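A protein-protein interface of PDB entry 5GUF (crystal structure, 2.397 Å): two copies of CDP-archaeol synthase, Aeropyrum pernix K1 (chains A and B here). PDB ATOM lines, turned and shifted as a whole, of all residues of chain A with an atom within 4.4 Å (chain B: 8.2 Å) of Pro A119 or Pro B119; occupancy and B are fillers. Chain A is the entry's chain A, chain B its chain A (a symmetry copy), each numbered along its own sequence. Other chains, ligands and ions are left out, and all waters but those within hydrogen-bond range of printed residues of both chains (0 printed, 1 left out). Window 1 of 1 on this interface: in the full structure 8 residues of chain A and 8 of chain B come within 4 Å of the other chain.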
ATOM      1  N   LEU A 110      13.291 -10.728  25.394  1.00  0.00           N
ATOM      2  CA  LEU A 110      12.819  -9.629  26.222  1.00  0.00           C
ATOM      3  C   LEU A 110      12.677 -10.017  27.689  1.00  0.00           C
ATOM      4  O   LEU A 110      12.174  -9.212  28.486  1.00  0.00           O
ATOM      5  CB  LEU A 110      11.481  -9.126  25.690  1.00  0.00           C
ATOM      6  CG  LEU A 110      11.533  -8.486  24.312  1.00  0.00           C
ATOM      7  CD1 LEU A 110      10.121  -8.195  23.871  1.00  0.00           C
ATOM      8  CD2 LEU A 110      12.363  -7.213  24.341  1.00  0.00           C
ATOM      9  N   ILE A 112      10.606 -12.325  28.802  1.00  0.00           N
ATOM     10  CA  ILE A 112       9.250 -12.775  29.101  1.00  0.00           C
ATOM     11  C   ILE A 112       9.251 -14.294  29.207  1.00  0.00           C
ATOM     12  O   ILE A 112       9.523 -14.989  28.222  1.00  0.00           O
ATOM     13  CB  ILE A 112       8.261 -12.305  28.032  1.00  0.00           C
ATOM     14  CG1 ILE A 112       8.269 -10.771  27.885  1.00  0.00           C
ATOM     15  CG2 ILE A 112       6.905 -12.755  28.394  1.00  0.00           C
ATOM     16  CD1 ILE A 112       7.478 -10.268  26.647  1.00  0.00           C
ATOM     17  N   PRO A 117       1.744 -13.790  29.236  1.00  0.00           N
ATOM     18  CA  PRO A 117       1.060 -13.159  28.088  1.00  0.00           C
ATOM     19  C   PRO A 117       1.847 -12.006  27.477  1.00  0.00           C
ATOM     20  O   PRO A 117       2.340 -11.129  28.187  1.00  0.00           O
ATOM     21  CB  PRO A 117      -0.260 -12.662  28.691  1.00  0.00           C
ATOM     22  CG  PRO A 117       0.054 -12.476  30.161  1.00  0.00           C
ATOM     23  CD  PRO A 117       1.057 -13.526  30.513  1.00  0.00           C
ATOM     24  N   ALA A 118       1.961 -12.021  26.147  1.00  0.00           N
ATOM     25  CA  ALA A 118       2.360 -10.856  25.356  1.00  0.00           C
ATOM     26  C   ALA A 118       1.171 -10.505  24.473  1.00  0.00           C
ATOM     27  O   ALA A 118       1.072 -10.992  23.335  1.00  0.00           O
ATOM     28  CB  ALA A 118       3.603 -11.142  24.520  1.00  0.00           C
ATOM     29  N   PRO A 119       0.235  -9.683  24.955  1.00  0.00           N
ATOM     30  CA  PRO A 119      -0.984  -9.430  24.177  1.00  0.00           C
ATOM     31  C   PRO A 119      -0.648  -8.778  22.842  1.00  0.00           C
ATOM     32  O   PRO A 119       0.364  -8.082  22.704  1.00  0.00           O
ATOM     33  CB  PRO A 119      -1.792  -8.491  25.080  1.00  0.00           C
ATOM     34  CG  PRO A 119      -0.756  -7.755  25.832  1.00  0.00           C
ATOM     35  CD  PRO A 119       0.343  -8.767  26.100  1.00  0.00           C
ATOM     36  N   LEU A 120      -1.502  -9.036  21.854  1.00  0.00           N
ATOM     37  CA  LEU A 120      -1.245  -8.696  20.457  1.00  0.00           C
ATOM     38  C   LEU A 120      -0.216  -9.645  19.849  1.00  0.00           C
ATOM     39  O   LEU A 120      -0.556 -10.404  18.940  1.00  0.00           O
ATOM     40  CB  LEU A 120      -0.804  -7.240  20.295  1.00  0.00           C
ATOM     41  CG  LEU A 120      -1.889  -6.181  20.492  1.00  0.00           C
ATOM     42  CD1 LEU A 120      -1.439  -4.874  19.837  1.00  0.00           C
ATOM     43  CD2 LEU A 120      -3.285  -6.631  19.975  1.00  0.00           C
ATOM     44  N   LEU A 121       1.030  -9.631  20.340  1.00  0.00           N
ATOM     45  CA  LEU A 121       2.056 -10.495  19.753  1.00  0.00           C
ATOM     46  C   LEU A 121       1.665 -11.970  19.827  1.00  0.00           C
ATOM     47  O   LEU A 121       1.818 -12.704  18.844  1.00  0.00           O
ATOM     48  CB  LEU A 121       3.405 -10.264  20.438  1.00  0.00           C
ATOM     49  CG  LEU A 121       4.581 -11.134  19.955  1.00  0.00           C
ATOM     50  CD1 LEU A 121       4.891 -10.898  18.461  1.00  0.00           C
ATOM     51  CD2 LEU A 121       5.837 -10.932  20.793  1.00  0.00           C
ATOM     52  N   GLN A 123      -1.200 -13.242  19.758  1.00  0.00           N
ATOM     53  CA  GLN A 123      -2.327 -13.582  18.906  1.00  0.00           C
ATOM     54  C   GLN A 123      -2.031 -13.378  17.426  1.00  0.00           C
ATOM     55  O   GLN A 123      -2.722 -13.958  16.591  1.00  0.00           O
ATOM     56  CB  GLN A 123      -3.560 -12.759  19.290  1.00  0.00           C
ATOM     57  CG  GLN A 123      -4.117 -13.025  20.681  1.00  0.00           C
ATOM     58  CD  GLN A 123      -3.323 -12.340  21.789  1.00  0.00           C
ATOM     59  OE1 GLN A 123      -2.725 -11.274  21.590  1.00  0.00           O
ATOM     60  NE2 GLN A 123      -3.311 -12.959  22.969  1.00  0.00           N
ATOM     61  N   GLY B 103      -3.622   0.755  27.555  1.00  0.00           N
ATOM     62  CA  GLY B 103      -2.676  -0.336  27.414  1.00  0.00           C
ATOM     63  C   GLY B 103      -2.119  -0.802  28.749  1.00  0.00           C
ATOM     64  O   GLY B 103      -1.970  -2.001  28.980  1.00  0.00           O
ATOM     65  N   VAL B 106      -4.706  -2.855  30.434  1.00  0.00           N
ATOM     66  CA  VAL B 106      -4.769  -4.217  29.924  1.00  0.00           C
ATOM     67  C   VAL B 106      -3.601  -5.038  30.456  1.00  0.00           C
ATOM     68  O   VAL B 106      -3.771  -6.206  30.823  1.00  0.00           O
ATOM     69  CB  VAL B 106      -4.842  -4.200  28.381  1.00  0.00           C
ATOM     70  CG1 VAL B 106      -4.452  -5.541  27.780  1.00  0.00           C
ATOM     71  CG2 VAL B 106      -6.261  -3.822  27.923  1.00  0.00           C
ATOM     72  N   LYS B 107      -2.418  -4.429  30.582  1.00  0.00           N
ATOM     73  CA  LYS B 107      -1.271  -5.172  31.103  1.00  0.00           C
ATOM     74  C   LYS B 107      -1.496  -5.604  32.546  1.00  0.00           C
ATOM     75  O   LYS B 107      -1.155  -6.736  32.924  1.00  0.00           O
ATOM     76  CB  LYS B 107       0.011  -4.344  31.005  1.00  0.00           C
ATOM     77  CG  LYS B 107       0.508  -4.087  29.596  1.00  0.00           C
ATOM     78  CD  LYS B 107       1.657  -3.120  29.604  1.00  0.00           C
ATOM     79  CE  LYS B 107       2.947  -3.807  29.987  1.00  0.00           C
ATOM     80  NZ  LYS B 107       4.088  -2.867  29.881  1.00  0.00           N
ATOM     81  N   LEU B 110      -3.784  -8.536  32.956  1.00  0.00           N
ATOM     82  CA  LEU B 110      -3.155  -9.774  32.525  1.00  0.00           C
ATOM     83  C   LEU B 110      -2.053 -10.235  33.471  1.00  0.00           C
ATOM     84  O   LEU B 110      -1.354 -11.211  33.164  1.00  0.00           O
ATOM     85  CB  LEU B 110      -2.586  -9.597  31.120  1.00  0.00           C
ATOM     86  CG  LEU B 110      -3.621  -9.369  30.029  1.00  0.00           C
ATOM     87  CD1 LEU B 110      -2.894  -9.055  28.746  1.00  0.00           C
ATOM     88  CD2 LEU B 110      -4.505 -10.594  29.862  1.00  0.00           C
ATOM     89  N   ILE B 112       0.702  -8.530  34.075  1.00  0.00           N
ATOM     90  CA  ILE B 112       2.006  -8.035  33.648  1.00  0.00           C
ATOM     91  C   ILE B 112       2.404  -6.867  34.541  1.00  0.00           C
ATOM     92  O   ILE B 112       1.739  -5.825  34.539  1.00  0.00           O
ATOM     93  CB  ILE B 112       1.986  -7.613  32.178  1.00  0.00           C
ATOM     94  CG1 ILE B 112       1.554  -8.772  31.259  1.00  0.00           C
ATOM     95  CG2 ILE B 112       3.330  -7.152  31.786  1.00  0.00           C
ATOM     96  CD1 ILE B 112       1.272  -8.327  29.798  1.00  0.00           C
ATOM     97  N   ARG B 116       7.269  -4.141  32.740  1.00  0.00           N
ATOM     98  CA  ARG B 116       7.671  -5.336  32.002  1.00  0.00           C
ATOM     99  C   ARG B 116       7.201  -5.176  30.580  1.00  0.00           C
ATOM    100  O   ARG B 116       6.179  -4.616  30.347  1.00  0.00           O
ATOM    101  CB  ARG B 116       7.145  -6.599  32.648  1.00  0.00           C
ATOM    102  CG  ARG B 116       8.228  -7.522  33.141  1.00  0.00           C
ATOM    103  CD  ARG B 116       9.062  -6.933  34.269  1.00  0.00           C
ATOM    104  NE  ARG B 116      10.363  -6.430  33.818  1.00  0.00           N
ATOM    105  CZ  ARG B 116      11.124  -6.983  32.868  1.00  0.00           C
ATOM    106  NH1 ARG B 116      10.745  -8.085  32.234  1.00  0.00           N
ATOM    107  NH2 ARG B 116      12.278  -6.424  32.552  1.00  0.00           N
ATOM    108  N   PRO B 117       7.965  -5.652  29.621  1.00  0.00           N
ATOM    109  CA  PRO B 117       7.629  -5.383  28.207  1.00  0.00           C
ATOM    110  C   PRO B 117       6.407  -6.150  27.721  1.00  0.00           C
ATOM    111  O   PRO B 117       6.285  -7.355  27.944  1.00  0.00           O
ATOM    112  CB  PRO B 117       8.890  -5.827  27.454  1.00  0.00           C
ATOM    113  CG  PRO B 117       9.525  -6.852  28.370  1.00  0.00           C
ATOM    114  CD  PRO B 117       9.217  -6.416  29.766  1.00  0.00           C
ATOM    115  N   ALA B 118       5.499  -5.434  27.055  1.00  0.00           N
ATOM    116  CA  ALA B 118       4.453  -6.028  26.220  1.00  0.00           C
ATOM    117  C   ALA B 118       4.723  -5.568  24.795  1.00  0.00           C
ATOM    118  O   ALA B 118       4.198  -4.529  24.364  1.00  0.00           O
ATOM    119  CB  ALA B 118       3.060  -5.610  26.680  1.00  0.00           C
ATOM    120  N   PRO B 119       5.548  -6.292  24.033  1.00  0.00           N
ATOM    121  CA  PRO B 119       5.928  -5.803  22.702  1.00  0.00           C
ATOM    122  C   PRO B 119       4.704  -5.671  21.806  1.00  0.00           C
ATOM    123  O   PRO B 119       3.705  -6.377  21.974  1.00  0.00           O
ATOM    124  CB  PRO B 119       6.892  -6.880  22.192  1.00  0.00           C
ATOM    125  CG  PRO B 119       6.418  -8.113  22.852  1.00  0.00           C
ATOM    126  CD  PRO B 119       5.978  -7.683  24.240  1.00  0.00           C
ATOM    127  N   LEU B 120       4.791  -4.735  20.863  1.00  0.00           N
ATOM    128  CA  LEU B 120       3.656  -4.298  20.053  1.00  0.00           C
ATOM    129  C   LEU B 120       2.711  -3.423  20.872  1.00  0.00           C
ATOM    130  O   LEU B 120       2.568  -2.239  20.567  1.00  0.00           O
ATOM    131  CB  LEU B 120       2.906  -5.481  19.438  1.00  0.00           C
ATOM    132  CG  LEU B 120       3.614  -6.208  18.294  1.00  0.00           C
ATOM    133  CD1 LEU B 120       2.583  -7.002  17.490  1.00  0.00           C
ATOM    134  CD2 LEU B 120       4.442  -5.256  17.384  1.00  0.00           C
ATOM    135  N   LEU B 121       2.074  -3.976  21.913  1.00  0.00           N
ATOM    136  CA  LEU B 121       1.126  -3.181  22.694  1.00  0.00           C
ATOM    137  C   LEU B 121       1.788  -1.944  23.302  1.00  0.00           C
ATOM    138  O   LEU B 121       1.222  -0.846  23.248  1.00  0.00           O
ATOM    139  CB  LEU B 121       0.484  -4.037  23.789  1.00  0.00           C
ATOM    140  CG  LEU B 121      -0.511  -3.326  24.724  1.00  0.00           C
ATOM    141  CD1 LEU B 121      -1.724  -2.765  23.950  1.00  0.00           C
ATOM    142  CD2 LEU B 121      -0.981  -4.223  25.863  1.00  0.00           C
ATOM    143  N   ASP B 122       2.989  -2.104  23.883  1.00  0.00           N
ATOM    144  CA  ASP B 122       3.705  -0.972  24.475  1.00  0.00           C
ATOM    145  C   ASP B 122       4.008   0.113  23.445  1.00  0.00           C
ATOM    146  O   ASP B 122       4.124   1.290  23.796  1.00  0.00           O
ATOM    147  CB  ASP B 122       5.027  -1.436  25.098  1.00  0.00           C
ATOM    148  CG  ASP B 122       4.851  -2.090  26.468  1.00  0.00           C
ATOM    149  OD1 ASP B 122       3.756  -1.964  27.058  1.00  0.00           O
ATOM    150  OD2 ASP B 122       5.811  -2.758  26.936  1.00  0.00           O
ATOM    151  N   GLN B 123       4.179  -0.255  22.182  1.00  0.00           N
ATOM    152  CA  GLN B 123       4.574   0.733  21.192  1.00  0.00           C
ATOM    153  C   GLN B 123       3.388   1.315  20.433  1.00  0.00           C
ATOM    154  O   GLN B 123       3.516   2.391  19.855  1.00  0.00           O
ATOM    155  CB  GLN B 123       5.561   0.126  20.190  1.00  0.00           C
ATOM    156  CG  GLN B 123       6.902  -0.300  20.770  1.00  0.00           C
ATOM    157  CD  GLN B 123       6.842  -1.634  21.508  1.00  0.00           C
ATOM    158  OE1 GLN B 123       6.036  -2.516  21.182  1.00  0.00           O
ATOM    159  NE2 GLN B 123       7.700  -1.784  22.516  1.00  0.00           N
ATOM    160  N   LEU B 124       2.234   0.656  20.442  1.00  0.00           N
ATOM    161  CA  LEU B 124       1.147   1.034  19.558  1.00  0.00           C
ATOM    162  C   LEU B 124      -0.106   1.537  20.273  1.00  0.00           C
ATOM    163  O   LEU B 124      -0.959   2.148  19.617  1.00  0.00           O
ATOM    164  CB  LEU B 124       0.788  -0.149  18.652  1.00  0.00           C
ATOM    165  CG  LEU B 124       1.860  -0.446  17.599  1.00  0.00           C
ATOM    166  CD1 LEU B 124       1.386  -1.513  16.628  1.00  0.00           C
ATOM    167  CD2 LEU B 124       2.261   0.831  16.848  1.00  0.00           C
ATOM    168  N   LEU B 154       6.859   1.682  15.097  1.00  0.00           N
ATOM    169  CA  LEU B 154       7.758   0.591  15.453  1.00  0.00           C
ATOM    170  C   LEU B 154       9.192   0.911  15.056  1.00  0.00           C
ATOM    171  O   LEU B 154      10.111   0.800  15.872  1.00  0.00           O
ATOM    172  CB  LEU B 154       7.301  -0.710  14.796  1.00  0.00           C
ATOM    173  CG  LEU B 154       5.918  -1.188  15.223  1.00  0.00           C
ATOM    174  CD1 LEU B 154       5.538  -2.437  14.450  1.00  0.00           C
ATOM    175  CD2 LEU B 154       5.907  -1.434  16.727  1.00  0.00           C
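The backbone NH (N) of Ile B112 is in hydrogen-bond range of the backbone carbonyl oxygen (O) of Lys B107 (2.8 Å).
CG of Pro B117 touches O of Leu A110, at 3.5 Å. Pro B119 touches Leu A110. Pro B119 touches Ile A112 (CD to CD1, 3.8 Å). CG of Pro A117 touches O of Leu B110 (3.5 Å). O of Pro A117 touches CD1 of Ile B112, 3.4 Å away. CG of Pro A119 touches CD1 of Leu B110, 3.8 Å away. CD1 of Ile B112 touches CD of Pro A119, 3.8 Å away. Pro A119 touches Pro B119. CD2 of Leu B121 touches CG of Pro A119, 3.5 Å away. CG of Pro B119 touches CD2 of Leu A121, 3.5 Å away.
Of the printed residues of chain A, Pro B119 touches Leu A110 (3.8 Å), Ile A112 (3.8 Å), Pro A119 (3.8 Å) and Leu A121 (3.5 Å). Of the printed residues of chain B, Ile A112 touches Pro B117 (3.4 Å) and Pro B119 (3.8 Å). Of the printed residues of chain A, Leu B110 touches Pro A117 and Pro A119. Of the printed residues of chain A, Pro B117 touches Leu A110 (3.5 Å) and Ile A112 (3.4 Å). Lys B107 touches none of the printed residues of chain A. Arg B116 touches none of the printed residues of chain A. The nearest residue of chain B that does not touch Pro A119 is Ala B118 (4.2 Å). The nearest residue of chain A that does not touch Pro B119 is Ala A118 (4.2 Å).
Along chain B the printed residues that touch a printed residue of chain A span positions 110 to 121. Of the 8 printed residues of chain A, 5 touch a printed residue of chain B. Hydrophobic or aromatic side chains of chain A within 4 Å of the printed part of chain B: Leu A110, Ile A112, Pro A117, Pro A119 and Leu A121.
Leu A110 touches Pro B117, and with the chains exchanged Pro A117 touches Leu B110. Ile A112 touches Pro B119, and with the chains exchanged Pro A119 touches Ile B112. Pro B119 touches its own counterpart, Pro A119. Pro A119 touches Leu B121, and with the chains exchanged Leu A121 touches Pro B119. Positions printed for both chains: 110, 112, 117, 118, 119, 120, 121 and 123. Of the 11 pairs that touch across the chains among the printed residues, 11 have their exchanged pair printed and touching as well.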
